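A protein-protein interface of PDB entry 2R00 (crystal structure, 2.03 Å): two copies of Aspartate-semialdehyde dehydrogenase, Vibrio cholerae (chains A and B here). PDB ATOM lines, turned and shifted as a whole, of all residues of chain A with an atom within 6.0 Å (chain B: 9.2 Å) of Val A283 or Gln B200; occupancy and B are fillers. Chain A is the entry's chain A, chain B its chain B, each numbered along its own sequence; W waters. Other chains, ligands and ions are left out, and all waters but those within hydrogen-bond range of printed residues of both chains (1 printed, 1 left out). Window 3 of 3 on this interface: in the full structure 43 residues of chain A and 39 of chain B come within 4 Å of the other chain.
No position is printed for both chains.
Of the 10 pairs that touch across the chains among the printed residues, none has its exchanged pair printed and touching as well.
Hydrophobic or aromatic side chains of chain A that line the printed part of chain B: Phe A274, Ala A277 and Val A283.
Among the printed residues, pairs that only touch across the chains: Phe A274 with Phe B195 (3.8 Å), Phe A274 with Ile B198 (3.5 Å), Phe A274 with Gln B200 (3.5 Å), Gly A276 with Gln B200 (3.6 Å), Val A283 with Gln B200 (3.5 Å), Val A283 with Ile B201 (3.7 Å), Arg A284 with Phe B195 (3.4 Å) and Asp A285 with Phe B195 (3.6 Å).
Water W1 bridges the backbone NH of Gly A276 (3.2 Å) and the side-chain amide oxygen of Gln B200 (3.2 Å).
Printed residues of chain B within 4 Å of Phe A274: Phe B195 (3.8 Å), Ile B198 (3.5 Å) and Gln B200 (3.5 Å).
Of chain B, only Gln B200 (2.7 Å) comes within 4 Å of Ala A277.
Asp A278 touches none of the printed residues of chain B.
Thr A281 touches none of the printed residues of chain B.
Of the printed residues of chain B, Val A283 touches Gln B200 (3.5 Å) and Ile B201 (3.7 Å).
Of the printed residues of chain B, Arg A284 touches Phe B195 and Gln B200.
Of the printed residues of chain B, Asp A285 touches Phe B195.
Of the printed residues of chain A, Phe B195 touches Phe A274, Arg A284 and Asp A285.
Of chain A, only Phe A274, Gly A276, Ala A277, Val A283 and Arg A284 come within 4 Å of Gln B200.
Of the printed residues of chain A, Ile B201 touches Val A283.
The nearest residue of chain B that does not touch Val A283 is Phe B195 (6.2 Å).
The nearest residue of chain A that does not touch Gln B200 is Gln A282 (4.1 Å).
The nearest printed residue of chain B that does not touch Asp A285 is Gln B200 (5.1 Å).
The backbone NH of Ala A277 lies within hydrogen-bond range of the backbone carbonyl oxygen of Gln B200, at 2.7 Å.
O of Arg A284 is in hydrogen-bond range of NE2 of Gln B200 (2.8 Å).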
ATOM      1  N   PHE A 274       1.298  24.936  -9.266  1.00  0.00           N
ATOM      2  CA  PHE A 274       0.389  25.280  -8.181  1.00  0.00           C
ATOM      3  C   PHE A 274      -0.173  26.680  -8.430  1.00  0.00           C
ATOM      4  O   PHE A 274       0.572  27.670  -8.453  1.00  0.00           O
ATOM      5  CB  PHE A 274       1.119  25.233  -6.838  1.00  0.00           C
ATOM      6  CG  PHE A 274       1.609  23.870  -6.461  1.00  0.00           C
ATOM      7  CD1 PHE A 274       2.717  23.308  -7.098  1.00  0.00           C
ATOM      8  CD2 PHE A 274       0.979  23.152  -5.455  1.00  0.00           C
ATOM      9  CE1 PHE A 274       3.170  22.046  -6.751  1.00  0.00           C
ATOM     10  CE2 PHE A 274       1.426  21.890  -5.097  1.00  0.00           C
ATOM     11  CZ  PHE A 274       2.522  21.331  -5.752  1.00  0.00           C
ATOM     12  N   GLY A 276      -2.552  28.017  -6.563  1.00  0.00           N
ATOM     13  CA  GLY A 276      -2.978  28.582  -5.294  1.00  0.00           C
ATOM     14  C   GLY A 276      -4.326  28.025  -4.886  1.00  0.00           C
ATOM     15  O   GLY A 276      -5.111  27.575  -5.731  1.00  0.00           O
ATOM     16  N   ALA A 277      -4.587  28.045  -3.583  1.00  0.00           N
ATOM     17  CA  ALA A 277      -5.815  27.485  -3.034  1.00  0.00           C
ATOM     18  C   ALA A 277      -6.690  28.604  -2.492  1.00  0.00           C
ATOM     19  O   ALA A 277      -6.182  29.537  -1.865  1.00  0.00           O
ATOM     20  CB  ALA A 277      -5.489  26.492  -1.919  1.00  0.00           C
ATOM     21  N   ASP A 278      -7.997  28.502  -2.740  1.00  0.00           N
ATOM     22  CA  ASP A 278      -8.975  29.382  -2.106  1.00  0.00           C
ATOM     23  C   ASP A 278      -9.604  28.668  -0.904  1.00  0.00           C
ATOM     24  O   ASP A 278     -10.153  29.310  -0.005  1.00  0.00           O
ATOM     25  CB  ASP A 278     -10.057  29.803  -3.107  1.00  0.00           C
ATOM     26  CG  ASP A 278      -9.600  30.932  -4.040  1.00  0.00           C
ATOM     27  OD1 ASP A 278      -8.640  31.651  -3.706  1.00  0.00           O
ATOM     28  OD2 ASP A 278     -10.216  31.113  -5.109  1.00  0.00           O
ATOM     29  N   PHE A 279      -9.508  27.339  -0.905  1.00  0.00           N
ATOM     30  CA  PHE A 279     -10.092  26.481   0.130  1.00  0.00           C
ATOM     31  C   PHE A 279      -9.079  25.438   0.625  1.00  0.00           C
ATOM     32  O   PHE A 279      -8.209  25.026  -0.134  1.00  0.00           O
ATOM     33  CB  PHE A 279     -11.352  25.790  -0.411  1.00  0.00           C
ATOM     34  CG  PHE A 279     -12.477  26.738  -0.719  1.00  0.00           C
ATOM     35  CD1 PHE A 279     -12.558  27.364  -1.960  1.00  0.00           C
ATOM     36  CD2 PHE A 279     -13.460  27.012   0.243  1.00  0.00           C
ATOM     37  CE1 PHE A 279     -13.592  28.259  -2.244  1.00  0.00           C
ATOM     38  CE2 PHE A 279     -14.497  27.891  -0.030  1.00  0.00           C
ATOM     39  CZ  PHE A 279     -14.564  28.520  -1.277  1.00  0.00           C
ATOM     40  N   PRO A 280      -9.183  25.015   1.904  1.00  0.00           N
ATOM     41  CA  PRO A 280      -8.260  24.002   2.448  1.00  0.00           C
ATOM     42  C   PRO A 280      -8.073  22.748   1.575  1.00  0.00           C
ATOM     43  O   PRO A 280      -6.934  22.297   1.396  1.00  0.00           O
ATOM     44  CB  PRO A 280      -8.889  23.639   3.793  1.00  0.00           C
ATOM     45  CG  PRO A 280      -9.634  24.883   4.195  1.00  0.00           C
ATOM     46  CD  PRO A 280     -10.151  25.478   2.919  1.00  0.00           C
ATOM     47  N   THR A 281      -9.167  22.202   1.037  1.00  0.00           N
ATOM     48  CA  THR A 281      -9.104  20.983   0.209  1.00  0.00           C
ATOM     49  C   THR A 281      -8.323  21.151  -1.100  1.00  0.00           C
ATOM     50  O   THR A 281      -7.960  20.153  -1.735  1.00  0.00           O
ATOM     51  CB  THR A 281     -10.504  20.438  -0.137  1.00  0.00           C
ATOM     52  OG1 THR A 281     -11.279  21.463  -0.790  1.00  0.00           O
ATOM     53  CG2 THR A 281     -11.217  19.927   1.139  1.00  0.00           C
ATOM     54  N   GLN A 282      -8.071  22.399  -1.496  1.00  0.00           N
ATOM     55  CA  GLN A 282      -7.286  22.686  -2.705  1.00  0.00           C
ATOM     56  C   GLN A 282      -5.758  22.715  -2.487  1.00  0.00           C
ATOM     57  O   GLN A 282      -4.987  22.682  -3.452  1.00  0.00           O
ATOM     58  CB  GLN A 282      -7.769  23.982  -3.361  1.00  0.00           C
ATOM     59  CG  GLN A 282      -9.175  23.898  -3.968  1.00  0.00           C
ATOM     60  CD  GLN A 282      -9.737  25.263  -4.353  1.00  0.00           C
ATOM     61  OE1 GLN A 282      -9.238  26.298  -3.921  1.00  0.00           O
ATOM     62  NE2 GLN A 282     -10.784  25.263  -5.164  1.00  0.00           N
ATOM     63  N   VAL A 283      -5.325  22.774  -1.227  1.00  0.00           N
ATOM     64  CA  VAL A 283      -3.899  22.694  -0.894  1.00  0.00           C
ATOM     65  C   VAL A 283      -3.396  21.274  -1.205  1.00  0.00           C
ATOM     66  O   VAL A 283      -3.991  20.280  -0.760  1.00  0.00           O
ATOM     67  CB  VAL A 283      -3.627  23.050   0.597  1.00  0.00           C
ATOM     68  CG1 VAL A 283      -2.130  23.117   0.889  1.00  0.00           C
ATOM     69  CG2 VAL A 283      -4.305  24.361   0.980  1.00  0.00           C
ATOM     70  N   ARG A 284      -2.314  21.190  -1.973  1.00  0.00           N
ATOM     71  CA  ARG A 284      -1.748  19.897  -2.375  1.00  0.00           C
ATOM     72  C   ARG A 284      -0.367  19.671  -1.771  1.00  0.00           C
ATOM     73  O   ARG A 284       0.311  20.628  -1.392  1.00  0.00           O
ATOM     74  CB  ARG A 284      -1.651  19.796  -3.900  1.00  0.00           C
ATOM     75  CG  ARG A 284      -2.918  20.182  -4.645  1.00  0.00           C
ATOM     76  CD  ARG A 284      -2.997  19.522  -6.019  1.00  0.00           C
ATOM     77  NE  ARG A 284      -1.902  19.909  -6.914  1.00  0.00           N
ATOM     78  CZ  ARG A 284      -1.850  21.051  -7.596  1.00  0.00           C
ATOM     79  NH1 ARG A 284      -2.822  21.953  -7.485  1.00  0.00           N
ATOM     80  NH2 ARG A 284      -0.817  21.296  -8.387  1.00  0.00           N
ATOM     81  N   ASP A 285       0.043  18.408  -1.685  1.00  0.00           N
ATOM     82  CA  ASP A 285       1.398  18.070  -1.253  1.00  0.00           C
ATOM     83  C   ASP A 285       2.324  18.021  -2.475  1.00  0.00           C
ATOM     84  O   ASP A 285       1.868  18.216  -3.603  1.00  0.00           O
ATOM     85  CB  ASP A 285       1.415  16.751  -0.460  1.00  0.00           C
ATOM     86  CG  ASP A 285       1.369  15.516  -1.352  1.00  0.00           C
ATOM     87  OD1 ASP A 285       1.914  14.471  -0.929  1.00  0.00           O
ATOM     88  OD2 ASP A 285       0.801  15.576  -2.468  1.00  0.00           O
ATOM     89  N   PHE B 195       9.285  23.693   0.349  1.00  0.00           N
ATOM     90  CA  PHE B 195       7.989  23.526  -0.325  1.00  0.00           C
ATOM     91  C   PHE B 195       7.040  24.690  -0.018  1.00  0.00           C
ATOM     92  O   PHE B 195       6.131  24.992  -0.804  1.00  0.00           O
ATOM     93  CB  PHE B 195       7.353  22.185   0.065  1.00  0.00           C
ATOM     94  CG  PHE B 195       6.042  21.901  -0.629  1.00  0.00           C
ATOM     95  CD1 PHE B 195       5.969  21.829  -2.021  1.00  0.00           C
ATOM     96  CD2 PHE B 195       4.875  21.691   0.117  1.00  0.00           C
ATOM     97  CE1 PHE B 195       4.744  21.568  -2.664  1.00  0.00           C
ATOM     98  CE2 PHE B 195       3.653  21.419  -0.520  1.00  0.00           C
ATOM     99  CZ  PHE B 195       3.590  21.357  -1.907  1.00  0.00           C
ATOM    100  N   ASN B 196       7.277  25.347   1.117  1.00  0.00           N
ATOM    101  CA  ASN B 196       6.469  26.499   1.524  1.00  0.00           C
ATOM    102  C   ASN B 196       6.777  27.784   0.739  1.00  0.00           C
ATOM    103  O   ASN B 196       6.055  28.773   0.868  1.00  0.00           O
ATOM    104  CB  ASN B 196       6.541  26.707   3.043  1.00  0.00           C
ATOM    105  CG  ASN B 196       5.739  25.666   3.815  1.00  0.00           C
ATOM    106  OD1 ASN B 196       4.681  25.217   3.364  1.00  0.00           O
ATOM    107  ND2 ASN B 196       6.236  25.284   4.989  1.00  0.00           N
ATOM    108  N   CYS B 197       7.841  27.760  -0.080  1.00  0.00           N
ATOM    109  CA  CYS B 197       8.127  28.845  -1.033  1.00  0.00           C
ATOM    110  C   CYS B 197       7.131  28.838  -2.199  1.00  0.00           C
ATOM    111  O   CYS B 197       7.101  29.778  -2.996  1.00  0.00           O
ATOM    112  CB  CYS B 197       9.562  28.752  -1.576  1.00  0.00           C
ATOM    113  SG  CYS B 197      10.825  28.760  -0.290  1.00  0.00           S
ATOM    114  N   ILE B 198       6.368  27.746  -2.324  1.00  0.00           N
ATOM    115  CA  ILE B 198       5.174  27.708  -3.176  1.00  0.00           C
ATOM    116  C   ILE B 198       3.988  28.184  -2.306  1.00  0.00           C
ATOM    117  O   ILE B 198       3.558  27.466  -1.400  1.00  0.00           O
ATOM    118  CB  ILE B 198       4.919  26.288  -3.788  1.00  0.00           C
ATOM    119  CG1 ILE B 198       6.192  25.724  -4.453  1.00  0.00           C
ATOM    120  CG2 ILE B 198       3.781  26.330  -4.795  1.00  0.00           C
ATOM    121  CD1 ILE B 198       6.669  26.524  -5.655  1.00  0.00           C
ATOM    122  N   PRO B 199       3.494  29.415  -2.562  1.00  0.00           N
ATOM    123  CA  PRO B 199       2.598  30.141  -1.650  1.00  0.00           C
ATOM    124  C   PRO B 199       1.123  29.803  -1.814  1.00  0.00           C
ATOM    125  O   PRO B 199       0.311  30.692  -2.084  1.00  0.00           O
ATOM    126  CB  PRO B 199       2.852  31.607  -2.021  1.00  0.00           C
ATOM    127  CG  PRO B 199       3.201  31.573  -3.469  1.00  0.00           C
ATOM    128  CD  PRO B 199       3.801  30.212  -3.769  1.00  0.00           C
ATOM    129  N   GLN B 200       0.784  28.531  -1.617  1.00  0.00           N
ATOM    130  CA  GLN B 200      -0.556  28.005  -1.899  1.00  0.00           C
ATOM    131  C   GLN B 200      -1.709  28.685  -1.145  1.00  0.00           C
ATOM    132  O   GLN B 200      -2.841  28.663  -1.618  1.00  0.00           O
ATOM    133  CB  GLN B 200      -0.620  26.497  -1.606  1.00  0.00           C
ATOM    134  CG  GLN B 200       0.266  25.617  -2.485  1.00  0.00           C
ATOM    135  CD  GLN B 200      -0.055  24.145  -2.316  1.00  0.00           C
ATOM    136  OE1 GLN B 200      -1.105  23.676  -2.748  1.00  0.00           O
ATOM    137  NE2 GLN B 200       0.852  23.409  -1.675  1.00  0.00           N
ATOM    138  N   ILE B 201      -1.422  29.246   0.032  1.00  0.00           N
ATOM    139  CA  ILE B 201      -2.477  29.745   0.937  1.00  0.00           C
ATOM    140  C   ILE B 201      -2.461  31.269   1.158  1.00  0.00           C
ATOM    141  O   ILE B 201      -3.162  31.786   2.025  1.00  0.00           O
ATOM    142  CB  ILE B 201      -2.505  28.954   2.292  1.00  0.00           C
ATOM    143  CG1 ILE B 201      -1.245  29.219   3.130  1.00  0.00           C
ATOM    144  CG2 ILE B 201      -2.645  27.461   2.021  1.00  0.00           C
ATOM    145  CD1 ILE B 201      -1.383  28.833   4.627  1.00  0.00           C
ATOM    146  N   ASP B 202      -1.668  31.978   0.358  1.00  0.00           N
ATOM    147  CA  ASP B 202      -1.648  33.439   0.406  1.00  0.00           C
ATOM    148  C   ASP B 202      -2.807  33.997  -0.392  1.00  0.00           C
ATOM    149  O   ASP B 202      -3.256  33.382  -1.359  1.00  0.00           O
ATOM    150  CB  ASP B 202      -0.312  33.989  -0.111  1.00  0.00           C
ATOM    151  CG  ASP B 202       0.792  33.897   0.928  1.00  0.00           C
ATOM    152  OD1 ASP B 202       0.607  34.415   2.042  1.00  0.00           O
ATOM    153  OD2 ASP B 202       1.851  33.307   0.641  1.00  0.00           O
ATOM    154  N   GLN B 203      -3.312  35.150   0.017  1.00  0.00           N
ATOM    155  CA  GLN B 203      -4.407  35.764  -0.728  1.00  0.00           C
ATOM    156  C   GLN B 203      -3.866  36.773  -1.735  1.00  0.00           C
ATOM    157  O   GLN B 203      -3.226  37.754  -1.366  1.00  0.00           O
ATOM    158  CB  GLN B 203      -5.429  36.408   0.211  1.00  0.00           C
ATOM    159  CG  GLN B 203      -6.823  36.544  -0.416  1.00  0.00           C
ATOM    160  CD  GLN B 203      -7.825  37.163   0.536  1.00  0.00           C
ATOM    161  OE1 GLN B 203      -8.573  36.454   1.213  1.00  0.00           O
ATOM    162  NE2 GLN B 203      -7.829  38.494   0.612  1.00  0.00           N
ATOM    163  N   PHE B 204      -4.124  36.511  -3.009  1.00  0.00           N
ATOM    164  CA  PHE B 204      -3.623  37.360  -4.077  1.00  0.00           C
ATOM    165  C   PHE B 204      -4.704  38.270  -4.648  1.00  0.00           C
ATOM    166  O   PHE B 204      -5.864  37.861  -4.801  1.00  0.00           O
ATOM    167  CB  PHE B 204      -2.996  36.507  -5.190  1.00  0.00           C
ATOM    168  CG  PHE B 204      -1.799  35.710  -4.739  1.00  0.00           C
ATOM    169  CD1 PHE B 204      -0.538  36.293  -4.687  1.00  0.00           C
ATOM    170  CD2 PHE B 204      -1.937  34.377  -4.358  1.00  0.00           C
ATOM    171  CE1 PHE B 204       0.580  35.561  -4.252  1.00  0.00           C
ATOM    172  CE2 PHE B 204      -0.823  33.631  -3.934  1.00  0.00           C
ATOM    173  CZ  PHE B 204       0.435  34.225  -3.884  1.00  0.00           C
ATOM    174  N   VAL B 238       9.238  32.638   3.992  1.00  0.00           N
ATOM    175  CA  VAL B 238      10.143  31.491   3.827  1.00  0.00           C
ATOM    176  C   VAL B 238      10.879  31.696   2.497  1.00  0.00           C
ATOM    177  O   VAL B 238      10.257  32.030   1.491  1.00  0.00           O
ATOM    178  CB  VAL B 238       9.385  30.132   3.853  1.00  0.00           C
ATOM    179  CG1 VAL B 238       8.279  30.115   2.810  1.00  0.00           C
ATOM    180  CG2 VAL B 238      10.342  28.934   3.666  1.00  0.00           C
HETATM  181  O   HOH W   1      -2.539  25.224  -5.104  1.00  0.00           O
